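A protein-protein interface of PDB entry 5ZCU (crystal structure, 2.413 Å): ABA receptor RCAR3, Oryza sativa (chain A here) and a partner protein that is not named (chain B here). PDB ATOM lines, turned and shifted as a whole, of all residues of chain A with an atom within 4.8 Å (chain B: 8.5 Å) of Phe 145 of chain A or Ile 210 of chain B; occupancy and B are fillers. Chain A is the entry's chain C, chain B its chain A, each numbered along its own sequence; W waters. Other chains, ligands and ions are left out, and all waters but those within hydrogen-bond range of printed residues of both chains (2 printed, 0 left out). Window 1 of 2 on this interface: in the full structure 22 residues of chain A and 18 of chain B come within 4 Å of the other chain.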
ATOM      1  N   GLY A  72      15.543  16.011  22.251  1.00  0.00           N
ATOM      2  CA  GLY A  72      14.932  15.138  21.268  1.00  0.00           C
ATOM      3  C   GLY A  72      14.872  15.697  19.868  1.00  0.00           C
ATOM      4  O   GLY A  72      14.035  15.258  19.073  1.00  0.00           O
ATOM      5  N   LEU A  73      15.729  16.654  19.539  1.00  0.00           N
ATOM      6  CA  LEU A  73      15.727  17.327  18.252  1.00  0.00           C
ATOM      7  C   LEU A  73      17.134  17.338  17.674  1.00  0.00           C
ATOM      8  O   LEU A  73      18.113  17.149  18.403  1.00  0.00           O
ATOM      9  CB  LEU A  73      15.197  18.761  18.398  1.00  0.00           C
ATOM     10  CG  LEU A  73      13.718  18.832  18.788  1.00  0.00           C
ATOM     11  CD1 LEU A  73      13.320  20.252  19.167  1.00  0.00           C
ATOM     12  CD2 LEU A  73      12.840  18.302  17.665  1.00  0.00           C
ATOM     13  N   PRO A  74      17.269  17.558  16.361  1.00  0.00           N
ATOM     14  CA  PRO A  74      18.618  17.639  15.775  1.00  0.00           C
ATOM     15  C   PRO A  74      19.351  18.925  16.106  1.00  0.00           C
ATOM     16  O   PRO A  74      20.585  18.948  16.029  1.00  0.00           O
ATOM     17  CB  PRO A  74      18.364  17.520  14.264  1.00  0.00           C
ATOM     18  CG  PRO A  74      16.898  17.260  14.100  1.00  0.00           C
ATOM     19  CD  PRO A  74      16.217  17.703  15.343  1.00  0.00           C
ATOM     20  N   LEU A 103      19.922  24.290   8.389  1.00  0.00           N
ATOM     21  CA  LEU A 103      18.974  24.838   7.418  1.00  0.00           C
ATOM     22  C   LEU A 103      19.487  26.220   7.017  1.00  0.00           C
ATOM     23  O   LEU A 103      19.173  27.221   7.661  1.00  0.00           O
ATOM     24  CB  LEU A 103      17.559  24.911   7.990  1.00  0.00           C
ATOM     25  CG  LEU A 103      16.866  23.601   8.371  1.00  0.00           C
ATOM     26  CD1 LEU A 103      15.734  23.873   9.345  1.00  0.00           C
ATOM     27  CD2 LEU A 103      16.347  22.885   7.134  1.00  0.00           C
ATOM     28  N   GLU A 141      14.235  14.558   1.279  1.00  0.00           N
ATOM     29  CA  GLU A 141      14.492  14.447   2.711  1.00  0.00           C
ATOM     30  C   GLU A 141      14.343  15.795   3.403  1.00  0.00           C
ATOM     31  O   GLU A 141      13.736  15.883   4.477  1.00  0.00           O
ATOM     32  CB  GLU A 141      15.894  13.888   2.950  1.00  0.00           C
ATOM     33  CG  GLU A 141      16.038  12.403   2.690  1.00  0.00           C
ATOM     34  CD  GLU A 141      17.489  11.963   2.744  1.00  0.00           C
ATOM     35  OE1 GLU A 141      18.362  12.765   2.352  1.00  0.00           O
ATOM     36  OE2 GLU A 141      17.752  10.825   3.185  1.00  0.00           O
ATOM     37  N   THR A 142      14.899  16.853   2.807  1.00  0.00           N
ATOM     38  CA  THR A 142      14.849  18.171   3.430  1.00  0.00           C
ATOM     39  C   THR A 142      13.417  18.681   3.537  1.00  0.00           C
ATOM     40  O   THR A 142      13.018  19.221   4.576  1.00  0.00           O
ATOM     41  CB  THR A 142      15.714  19.159   2.648  1.00  0.00           C
ATOM     42  OG1 THR A 142      17.057  18.663   2.566  1.00  0.00           O
ATOM     43  CG2 THR A 142      15.729  20.510   3.341  1.00  0.00           C
ATOM     44  N   CYS A 143      12.632  18.532   2.467  1.00  0.00           N
ATOM     45  CA  CYS A 143      11.232  18.943   2.512  1.00  0.00           C
ATOM     46  C   CYS A 143      10.454  18.137   3.545  1.00  0.00           C
ATOM     47  O   CYS A 143       9.695  18.697   4.344  1.00  0.00           O
ATOM     48  CB  CYS A 143      10.598  18.793   1.128  1.00  0.00           C
ATOM     49  SG  CYS A 143      11.098  20.052  -0.071  1.00  0.00           S
ATOM     50  N   TYR A 144      10.639  16.814   3.546  1.00  0.00           N
ATOM     51  CA  TYR A 144       9.932  15.959   4.496  1.00  0.00           C
ATOM     52  C   TYR A 144      10.276  16.324   5.934  1.00  0.00           C
ATOM     53  O   TYR A 144       9.412  16.287   6.817  1.00  0.00           O
ATOM     54  CB  TYR A 144      10.268  14.495   4.221  1.00  0.00           C
ATOM     55  CG  TYR A 144       9.421  13.496   4.976  1.00  0.00           C
ATOM     56  CD1 TYR A 144       9.745  13.117   6.272  1.00  0.00           C
ATOM     57  CD2 TYR A 144       8.300  12.926   4.388  1.00  0.00           C
ATOM     58  CE1 TYR A 144       8.976  12.204   6.965  1.00  0.00           C
ATOM     59  CE2 TYR A 144       7.527  12.008   5.071  1.00  0.00           C
ATOM     60  CZ  TYR A 144       7.867  11.651   6.356  1.00  0.00           C
ATOM     61  OH  TYR A 144       7.096  10.738   7.038  1.00  0.00           O
ATOM     62  N   PHE A 145      11.535  16.676   6.189  1.00  0.00           N
ATOM     63  CA  PHE A 145      11.952  17.026   7.542  1.00  0.00           C
ATOM     64  C   PHE A 145      11.334  18.346   7.985  1.00  0.00           C
ATOM     65  O   PHE A 145      10.827  18.459   9.108  1.00  0.00           O
ATOM     66  CB  PHE A 145      13.480  17.077   7.606  1.00  0.00           C
ATOM     67  CG  PHE A 145      14.028  17.780   8.814  1.00  0.00           C
ATOM     68  CD1 PHE A 145      13.801  17.284  10.088  1.00  0.00           C
ATOM     69  CD2 PHE A 145      14.792  18.924   8.672  1.00  0.00           C
ATOM     70  CE1 PHE A 145      14.315  17.929  11.197  1.00  0.00           C
ATOM     71  CE2 PHE A 145      15.309  19.573   9.775  1.00  0.00           C
ATOM     72  CZ  PHE A 145      15.070  19.076  11.040  1.00  0.00           C
ATOM     73  N   VAL A 146      11.361  19.357   7.113  1.00  0.00           N
ATOM     74  CA  VAL A 146      10.802  20.658   7.468  1.00  0.00           C
ATOM     75  C   VAL A 146       9.281  20.584   7.564  1.00  0.00           C
ATOM     76  O   VAL A 146       8.677  21.150   8.485  1.00  0.00           O
ATOM     77  CB  VAL A 146      11.256  21.730   6.459  1.00  0.00           C
ATOM     78  CG1 VAL A 146      10.571  23.055   6.758  1.00  0.00           C
ATOM     79  CG2 VAL A 146      12.770  21.886   6.488  1.00  0.00           C
ATOM     80  N   GLU A 147       8.639  19.901   6.612  1.00  0.00           N
ATOM     81  CA  GLU A 147       7.183  19.793   6.626  1.00  0.00           C
ATOM     82  C   GLU A 147       6.687  19.116   7.897  1.00  0.00           C
ATOM     83  O   GLU A 147       5.637  19.483   8.434  1.00  0.00           O
ATOM     84  CB  GLU A 147       6.697  19.033   5.392  1.00  0.00           C
ATOM     85  CG  GLU A 147       6.775  19.825   4.098  1.00  0.00           C
ATOM     86  CD  GLU A 147       6.566  18.955   2.874  1.00  0.00           C
ATOM     87  OE1 GLU A 147       7.280  19.157   1.869  1.00  0.00           O
ATOM     88  OE2 GLU A 147       5.689  18.067   2.918  1.00  0.00           O
ATOM     89  N   ALA A 148       7.423  18.117   8.389  1.00  0.00           N
ATOM     90  CA  ALA A 148       7.005  17.418   9.600  1.00  0.00           C
ATOM     91  C   ALA A 148       7.006  18.353  10.803  1.00  0.00           C
ATOM     92  O   ALA A 148       6.099  18.301  11.641  1.00  0.00           O
ATOM     93  CB  ALA A 148       7.913  16.213   9.852  1.00  0.00           C
ATOM     94  N   LEU A 149       8.022  19.211  10.907  1.00  0.00           N
ATOM     95  CA  LEU A 149       8.085  20.154  12.018  1.00  0.00           C
ATOM     96  C   LEU A 149       7.040  21.253  11.869  1.00  0.00           C
ATOM     97  O   LEU A 149       6.394  21.639  12.851  1.00  0.00           O
ATOM     98  CB  LEU A 149       9.489  20.749  12.116  1.00  0.00           C
ATOM     99  CG  LEU A 149      10.570  19.780  12.602  1.00  0.00           C
ATOM    100  CD1 LEU A 149      11.954  20.385  12.432  1.00  0.00           C
ATOM    101  CD2 LEU A 149      10.319  19.395  14.052  1.00  0.00           C
ATOM    102  N   HIS B  63      12.533  12.827  26.630  1.00  0.00           N
ATOM    103  CA  HIS B  63      12.883  13.881  25.688  1.00  0.00           C
ATOM    104  C   HIS B  63      11.681  14.792  25.494  1.00  0.00           C
ATOM    105  O   HIS B  63      10.531  14.371  25.657  1.00  0.00           O
ATOM    106  CB  HIS B  63      13.349  13.320  24.336  1.00  0.00           C
ATOM    107  CG  HIS B  63      12.496  12.206  23.814  1.00  0.00           C
ATOM    108  ND1 HIS B  63      12.769  10.879  24.065  1.00  0.00           N
ATOM    109  CD2 HIS B  63      11.380  12.221  23.047  1.00  0.00           C
ATOM    110  CE1 HIS B  63      11.857  10.124  23.478  1.00  0.00           C
ATOM    111  NE2 HIS B  63      11.002  10.914  22.854  1.00  0.00           N
ATOM    112  N   ASN B 141       5.106  16.350  21.589  1.00  0.00           N
ATOM    113  CA  ASN B 141       6.520  16.103  21.334  1.00  0.00           C
ATOM    114  C   ASN B 141       7.258  15.503  22.524  1.00  0.00           C
ATOM    115  O   ASN B 141       8.477  15.318  22.443  1.00  0.00           O
ATOM    116  CB  ASN B 141       7.212  17.402  20.910  1.00  0.00           C
ATOM    117  CG  ASN B 141       7.234  18.440  22.014  1.00  0.00           C
ATOM    118  OD1 ASN B 141       6.245  18.631  22.720  1.00  0.00           O
ATOM    119  ND2 ASN B 141       8.366  19.113  22.173  1.00  0.00           N
ATOM    120  N   PRO B 183      17.079   4.532  14.370  1.00  0.00           N
ATOM    121  CA  PRO B 183      16.344   4.461  13.094  1.00  0.00           C
ATOM    122  C   PRO B 183      17.101   3.769  11.971  1.00  0.00           C
ATOM    123  O   PRO B 183      16.478   3.068  11.162  1.00  0.00           O
ATOM    124  CB  PRO B 183      16.076   5.940  12.772  1.00  0.00           C
ATOM    125  CG  PRO B 183      16.147   6.641  14.092  1.00  0.00           C
ATOM    126  CD  PRO B 183      17.178   5.906  14.887  1.00  0.00           C
ATOM    127  N   LYS B 198      10.114   7.853   6.568  1.00  0.00           N
ATOM    128  CA  LYS B 198      11.483   8.044   6.110  1.00  0.00           C
ATOM    129  C   LYS B 198      12.421   8.090   7.305  1.00  0.00           C
ATOM    130  O   LYS B 198      12.069   8.604   8.371  1.00  0.00           O
ATOM    131  CB  LYS B 198      11.638   9.334   5.290  1.00  0.00           C
ATOM    132  CG  LYS B 198      10.915   9.335   3.954  1.00  0.00           C
ATOM    133  CD  LYS B 198      10.757  10.754   3.436  1.00  0.00           C
ATOM    134  CE  LYS B 198      11.649  11.030   2.242  1.00  0.00           C
ATOM    135  NZ  LYS B 198      11.168  10.330   1.020  1.00  0.00           N
ATOM    136  N   VAL B 199      13.620   7.547   7.114  1.00  0.00           N
ATOM    137  CA  VAL B 199      14.715   7.685   8.066  1.00  0.00           C
ATOM    138  C   VAL B 199      15.768   8.573   7.421  1.00  0.00           C
ATOM    139  O   VAL B 199      16.332   8.220   6.378  1.00  0.00           O
ATOM    140  CB  VAL B 199      15.300   6.322   8.462  1.00  0.00           C
ATOM    141  CG1 VAL B 199      16.620   6.505   9.199  1.00  0.00           C
ATOM    142  CG2 VAL B 199      14.304   5.550   9.317  1.00  0.00           C
ATOM    143  N   ILE B 200      16.026   9.726   8.035  1.00  0.00           N
ATOM    144  CA  ILE B 200      16.898  10.748   7.470  1.00  0.00           C
ATOM    145  C   ILE B 200      18.084  10.964   8.397  1.00  0.00           C
ATOM    146  O   ILE B 200      17.922  11.043   9.619  1.00  0.00           O
ATOM    147  CB  ILE B 200      16.137  12.072   7.247  1.00  0.00           C
ATOM    148  CG1 ILE B 200      14.854  11.822   6.449  1.00  0.00           C
ATOM    149  CG2 ILE B 200      17.024  13.099   6.556  1.00  0.00           C
ATOM    150  CD1 ILE B 200      13.913  13.003   6.425  1.00  0.00           C
ATOM    151  N   GLN B 201      19.278  11.054   7.814  1.00  0.00           N
ATOM    152  CA  GLN B 201      20.466  11.438   8.565  1.00  0.00           C
ATOM    153  C   GLN B 201      20.496  12.956   8.706  1.00  0.00           C
ATOM    154  O   GLN B 201      20.606  13.679   7.709  1.00  0.00           O
ATOM    155  CB  GLN B 201      21.739  10.938   7.884  1.00  0.00           C
ATOM    156  CG  GLN B 201      23.009  11.539   8.473  1.00  0.00           C
ATOM    157  CD  GLN B 201      24.252  10.737   8.148  1.00  0.00           C
ATOM    158  OE1 GLN B 201      24.535  10.453   6.984  1.00  0.00           O
ATOM    159  NE2 GLN B 201      25.006  10.370   9.180  1.00  0.00           N
ATOM    160  N   TRP B 202      20.397  13.436   9.943  1.00  0.00           N
ATOM    161  CA  TRP B 202      20.308  14.871  10.224  1.00  0.00           C
ATOM    162  C   TRP B 202      20.839  15.058  11.645  1.00  0.00           C
ATOM    163  O   TRP B 202      20.081  14.983  12.616  1.00  0.00           O
ATOM    164  CB  TRP B 202      18.882  15.382  10.075  1.00  0.00           C
ATOM    165  CG  TRP B 202      18.785  16.846   9.754  1.00  0.00           C
ATOM    166  CD1 TRP B 202      18.983  17.890  10.614  1.00  0.00           C
ATOM    167  CD2 TRP B 202      18.459  17.431   8.486  1.00  0.00           C
ATOM    168  NE1 TRP B 202      18.807  19.085   9.959  1.00  0.00           N
ATOM    169  CE2 TRP B 202      18.484  18.832   8.652  1.00  0.00           C
ATOM    170  CE3 TRP B 202      18.153  16.908   7.226  1.00  0.00           C
ATOM    171  CZ2 TRP B 202      18.214  19.713   7.607  1.00  0.00           C
ATOM    172  CZ3 TRP B 202      17.883  17.785   6.190  1.00  0.00           C
ATOM    173  CH2 TRP B 202      17.917  19.172   6.386  1.00  0.00           C
ATOM    174  N   ASN B 203      22.145  15.321  11.743  1.00  0.00           N
ATOM    175  CA  ASN B 203      22.913  15.038  12.953  1.00  0.00           C
ATOM    176  C   ASN B 203      22.508  13.690  13.535  1.00  0.00           C
ATOM    177  O   ASN B 203      21.873  13.621  14.593  1.00  0.00           O
ATOM    178  CB  ASN B 203      22.730  16.152  13.988  1.00  0.00           C
ATOM    179  CG  ASN B 203      22.869  17.535  13.386  1.00  0.00           C
ATOM    180  OD1 ASN B 203      23.538  17.717  12.369  1.00  0.00           O
ATOM    181  ND2 ASN B 203      22.246  18.524  14.019  1.00  0.00           N
ATOM    182  N   GLY B 204      22.870  12.619  12.842  1.00  0.00           N
ATOM    183  CA  GLY B 204      22.475  11.275  13.201  1.00  0.00           C
ATOM    184  C   GLY B 204      21.219  10.834  12.465  1.00  0.00           C
ATOM    185  O   GLY B 204      20.435  11.640  11.960  1.00  0.00           O
ATOM    186  N   TYR B 205      21.034   9.518  12.400  1.00  0.00           N
ATOM    187  CA  TYR B 205      19.865   8.950  11.742  1.00  0.00           C
ATOM    188  C   TYR B 205      18.635   9.116  12.624  1.00  0.00           C
ATOM    189  O   TYR B 205      18.645   8.732  13.798  1.00  0.00           O
ATOM    190  CB  TYR B 205      20.106   7.478  11.414  1.00  0.00           C
ATOM    191  CG  TYR B 205      20.998   7.302  10.211  1.00  0.00           C
ATOM    192  CD1 TYR B 205      20.476   7.348   8.926  1.00  0.00           C
ATOM    193  CD2 TYR B 205      22.366   7.123  10.357  1.00  0.00           C
ATOM    194  CE1 TYR B 205      21.288   7.197   7.820  1.00  0.00           C
ATOM    195  CE2 TYR B 205      23.189   6.973   9.257  1.00  0.00           C
ATOM    196  CZ  TYR B 205      22.644   7.012   7.989  1.00  0.00           C
ATOM    197  OH  TYR B 205      23.454   6.866   6.888  1.00  0.00           O
ATOM    198  N   ARG B 206      17.575   9.690  12.055  1.00  0.00           N
ATOM    199  CA  ARG B 206      16.391  10.048  12.819  1.00  0.00           C
ATOM    200  C   ARG B 206      15.130   9.762  12.019  1.00  0.00           C
ATOM    201  O   ARG B 206      15.110   9.922  10.796  1.00  0.00           O
ATOM    202  CB  ARG B 206      16.418  11.526  13.226  1.00  0.00           C
ATOM    203  CG  ARG B 206      17.581  11.909  14.128  1.00  0.00           C
ATOM    204  CD  ARG B 206      17.718  13.416  14.229  1.00  0.00           C
ATOM    205  NE  ARG B 206      18.901  13.809  14.988  1.00  0.00           N
ATOM    206  CZ  ARG B 206      18.908  14.043  16.295  1.00  0.00           C
ATOM    207  NH1 ARG B 206      17.792  13.926  16.999  1.00  0.00           N
ATOM    208  NH2 ARG B 206      20.034  14.393  16.900  1.00  0.00           N
ATOM    209  N   VAL B 207      14.084   9.324  12.720  1.00  0.00           N
ATOM    210  CA  VAL B 207      12.767   9.198  12.107  1.00  0.00           C
ATOM    211  C   VAL B 207      12.287  10.581  11.695  1.00  0.00           C
ATOM    212  O   VAL B 207      12.238  11.505  12.518  1.00  0.00           O
ATOM    213  CB  VAL B 207      11.784   8.527  13.068  1.00  0.00           C
ATOM    214  CG1 VAL B 207      10.459   8.282  12.371  1.00  0.00           C
ATOM    215  CG2 VAL B 207      12.371   7.225  13.598  1.00  0.00           C
ATOM    216  N   SER B 208      11.939  10.732  10.416  1.00  0.00           N
ATOM    217  CA  SER B 208      11.558  12.017   9.829  1.00  0.00           C
ATOM    218  C   SER B 208      12.660  13.062   9.977  1.00  0.00           C
ATOM    219  O   SER B 208      12.400  14.262   9.860  1.00  0.00           O
ATOM    220  CB  SER B 208      10.251  12.550  10.431  1.00  0.00           C
ATOM    221  OG  SER B 208       9.292  11.518  10.569  1.00  0.00           O
ATOM    222  N   GLY B 209      13.890  12.625  10.234  1.00  0.00           N
ATOM    223  CA  GLY B 209      14.970  13.549  10.512  1.00  0.00           C
ATOM    224  C   GLY B 209      14.900  14.216  11.865  1.00  0.00           C
ATOM    225  O   GLY B 209      15.708  15.107  12.141  1.00  0.00           O
ATOM    226  N   ILE B 210      13.961  13.813  12.721  1.00  0.00           N
ATOM    227  CA  ILE B 210      13.709  14.475  13.999  1.00  0.00           C
ATOM    228  C   ILE B 210      14.205  13.634  15.176  1.00  0.00           C
ATOM    229  O   ILE B 210      15.093  14.055  15.917  1.00  0.00           O
ATOM    230  CB  ILE B 210      12.212  14.821  14.153  1.00  0.00           C
ATOM    231  CG1 ILE B 210      11.792  15.847  13.100  1.00  0.00           C
ATOM    232  CG2 ILE B 210      11.942  15.351  15.545  1.00  0.00           C
ATOM    233  CD1 ILE B 210      10.298  15.932  12.899  1.00  0.00           C
ATOM    234  N   LEU B 211      13.629  12.452  15.370  1.00  0.00           N
ATOM    235  CA  LEU B 211      13.844  11.666  16.579  1.00  0.00           C
ATOM    236  C   LEU B 211      14.878  10.577  16.336  1.00  0.00           C
ATOM    237  O   LEU B 211      14.745   9.784  15.398  1.00  0.00           O
ATOM    238  CB  LEU B 211      12.538  11.038  17.063  1.00  0.00           C
ATOM    239  CG  LEU B 211      12.583  10.503  18.495  1.00  0.00           C
ATOM    240  CD1 LEU B 211      12.871  11.632  19.476  1.00  0.00           C
ATOM    241  CD2 LEU B 211      11.276   9.799  18.846  1.00  0.00           C
ATOM    242  N   ALA B 212      15.882  10.518  17.209  1.00  0.00           N
ATOM    243  CA  ALA B 212      16.974   9.559  17.112  1.00  0.00           C
ATOM    244  C   ALA B 212      16.604   8.179  17.644  1.00  0.00           C
ATOM    245  O   ALA B 212      17.501   7.412  18.015  1.00  0.00           O
ATOM    246  CB  ALA B 212      18.204  10.089  17.853  1.00  0.00           C
ATOM    247  N   MET B 213      15.315   7.849  17.703  1.00  0.00           N
ATOM    248  CA  MET B 213      14.862   6.527  18.112  1.00  0.00           C
ATOM    249  C   MET B 213      13.651   6.133  17.280  1.00  0.00           C
ATOM    250  O   MET B 213      12.874   6.988  16.848  1.00  0.00           O
ATOM    251  CB  MET B 213      14.477   6.476  19.601  1.00  0.00           C
ATOM    252  CG  MET B 213      15.358   7.282  20.537  1.00  0.00           C
ATOM    253  SD  MET B 213      14.430   7.960  21.922  1.00  0.00           S
ATOM    254  CE  MET B 213      13.452   6.543  22.392  1.00  0.00           C
ATOM    255  N   ASP B 219       5.420  10.641  22.303  1.00  0.00           N
ATOM    256  CA  ASP B 219       5.704  11.211  20.982  1.00  0.00           C
ATOM    257  C   ASP B 219       4.596  10.902  19.976  1.00  0.00           C
ATOM    258  O   ASP B 219       4.833  10.344  18.902  1.00  0.00           O
ATOM    259  CB  ASP B 219       7.051  10.721  20.455  1.00  0.00           C
ATOM    260  CG  ASP B 219       8.173  10.890  21.457  1.00  0.00           C
ATOM    261  OD1 ASP B 219       8.611  12.039  21.676  1.00  0.00           O
ATOM    262  OD2 ASP B 219       8.629   9.871  22.016  1.00  0.00           O
ATOM    263  N   TYR B 221       3.087  12.743  17.990  1.00  0.00           N
ATOM    264  CA  TYR B 221       3.180  13.418  16.697  1.00  0.00           C
ATOM    265  C   TYR B 221       4.016  12.660  15.665  1.00  0.00           C
ATOM    266  O   TYR B 221       3.975  13.024  14.484  1.00  0.00           O
ATOM    267  CB  TYR B 221       3.720  14.840  16.883  1.00  0.00           C
ATOM    268  CG  TYR B 221       5.228  14.955  16.998  1.00  0.00           C
ATOM    269  CD1 TYR B 221       5.907  14.452  18.103  1.00  0.00           C
ATOM    270  CD2 TYR B 221       5.972  15.604  16.016  1.00  0.00           C
ATOM    271  CE1 TYR B 221       7.284  14.570  18.214  1.00  0.00           C
ATOM    272  CE2 TYR B 221       7.350  15.726  16.122  1.00  0.00           C
ATOM    273  CZ  TYR B 221       7.997  15.208  17.223  1.00  0.00           C
ATOM    274  OH  TYR B 221       9.363  15.325  17.341  1.00  0.00           O
ATOM    275  N   LEU B 222       4.757  11.624  16.071  1.00  0.00           N
ATOM    276  CA  LEU B 222       5.629  10.857  15.180  1.00  0.00           C
ATOM    277  C   LEU B 222       5.084   9.460  14.885  1.00  0.00           C
ATOM    278  O   LEU B 222       5.834   8.549  14.518  1.00  0.00           O
ATOM    279  CB  LEU B 222       7.025  10.743  15.773  1.00  0.00           C
ATOM    280  CG  LEU B 222       7.891  11.969  15.531  1.00  0.00           C
ATOM    281  CD1 LEU B 222       9.197  11.820  16.269  1.00  0.00           C
ATOM    282  CD2 LEU B 222       8.122  12.168  14.040  1.00  0.00           C
ATOM    283  N   VAL B 226       6.969   5.876  15.284  1.00  0.00           N
ATOM    284  CA  VAL B 226       7.594   5.588  16.573  1.00  0.00           C
ATOM    285  C   VAL B 226       6.579   4.820  17.410  1.00  0.00           C
ATOM    286  O   VAL B 226       5.558   5.377  17.827  1.00  0.00           O
ATOM    287  CB  VAL B 226       8.054   6.871  17.279  1.00  0.00           C
ATOM    288  CG1 VAL B 226       8.626   6.544  18.650  1.00  0.00           C
ATOM    289  CG2 VAL B 226       9.083   7.603  16.431  1.00  0.00           C
HETATM  290  O   HOH W   1       8.691   9.262   8.977  1.00  0.00           O
HETATM  291  O   HOH W   2      16.067  12.563  19.494  1.00  0.00           O
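ND2 of Asn 203 of chain B is in hydrogen-bond range of O of Pro 74 of chain A (2.6 Å).
A ring nitrogen (NE2) of His 63 of chain B sits at hydrogen-bond distance from the side-chain carboxylate (OD2) of Asp 219 of chain B (2.7 Å). The backbone carbonyl oxygen (O) of Lys 198 of chain B lies within hydrogen-bond range of the backbone NH (N) of Ser 208 of chain B, at 3.0 Å. O of Ile 200 of chain B lies within hydrogen-bond range of N of Arg 206 of chain B (2.8 Å). The backbone carbonyl oxygen (O) of Trp 202 of chain B is in hydrogen-bond range of the guanidinium group (NE) of Arg 206 of chain B, at 2.9 Å. O of Asn 203 of chain B is in hydrogen-bond range of NE of Arg 206 of chain B (3.0 Å). O of Ile 210 of chain B is in hydrogen-bond range of NH1 of Arg 206 of chain B (2.9 Å).
Among the printed residues, merely in contact across the chains: Pro 74 of chain A with Gly 209 of chain B (3.1 Å), Phe 145 of chain A with Gly 209 of chain B (3.3 Å), Phe 145 of chain A with Ser 208 of chain B (3.3 Å), Tyr 144 of chain A with Lys 198 of chain B (3.4 Å), Phe 145 of chain A with Trp 202 of chain B (3.4 Å), Pro 74 of chain A with Trp 202 of chain B (3.5 Å), Glu 141 of chain A with Ile 200 of chain B (3.5 Å), Leu 73 of chain A with Arg 206 of chain B (3.5 Å), Gly 72 of chain A with Ile 210 of chain B (3.5 Å), Pro 74 of chain A with Arg 206 of chain B (3.6 Å), Leu 149 of chain A with Ile 210 of chain B (3.6 Å), Tyr 144 of chain A with Ser 208 of chain B (3.7 Å), Leu 103 of chain A with Trp 202 of chain B (3.7 Å), Leu 73 of chain A with Ile 210 of chain B (3.7 Å), Phe 145 of chain A with Ile 210 of chain B (3.8 Å), Thr 142 of chain A with Trp 202 of chain B (3.8 Å), Gly 72 of chain A with Leu 211 of chain B (3.8 Å), Pro 74 of chain A with Ile 210 of chain B (3.9 Å), Ala 148 of chain A with Ile 210 of chain B (3.9 Å) and Gly 72 of chain A with His 63 of chain B (3.9 Å).
Phe 145 of chain A touches just these residues of chain B: Trp 202, Ser 208, Gly 209 and Ile 210. Of the printed residues of chain A, Ile 200 of chain B touches Glu 141. Printed residues of chain A within 4 Å of Asn 203 of chain B: Pro 74. Gly 204 of chain B touches none of the printed residues of chain A. Ile 210 of chain B touches just these residues of chain A: Gly 72 (3.5 Å), Leu 73 (3.7 Å), Pro 74 (3.9 Å), Phe 145 (3.8 Å), Ala 148 (3.9 Å) and Leu 149 (3.6 Å). Tyr 221 of chain B touches none of the printed residues of chain A. The nearest printed residue of chain A that does not touch Ile 210 of chain B is Tyr 144 of chain A (6.2 Å). The nearest printed residue of chain B that does not touch Thr 142 of chain A is Ile 200 of chain B (5.4 Å).
Printed residues of chain A that touch a printed residue of chain B: Gly 72, Leu 73, Pro 74, Leu 103, Glu 141, Thr 142, Tyr 144, Phe 145, Ala 148 and Leu 149. Of the 23 printed residues of chain B, 10 touch a printed residue of chain A. Among the printed residues, no Asp or Glu carboxylate lies within 4 Å of a Lys or Arg side-chain nitrogen of the other chain.
Water W1 lies within hydrogen-bond range of the side-chain hydroxyl of Ser 208 of chain B (2.8 Å), the side-chain hydroxyl of Tyr 144 of chain A (2.9 Å) and the backbone NH of Lys 198 of chain B (3.1 Å). Water W2 lies within hydrogen-bond range of N of Ala 212 of chain B (3.1 Å), NH1 of Arg 206 of chain B (3.3 Å) and O of Gly 72 of chain A (3.4 Å).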
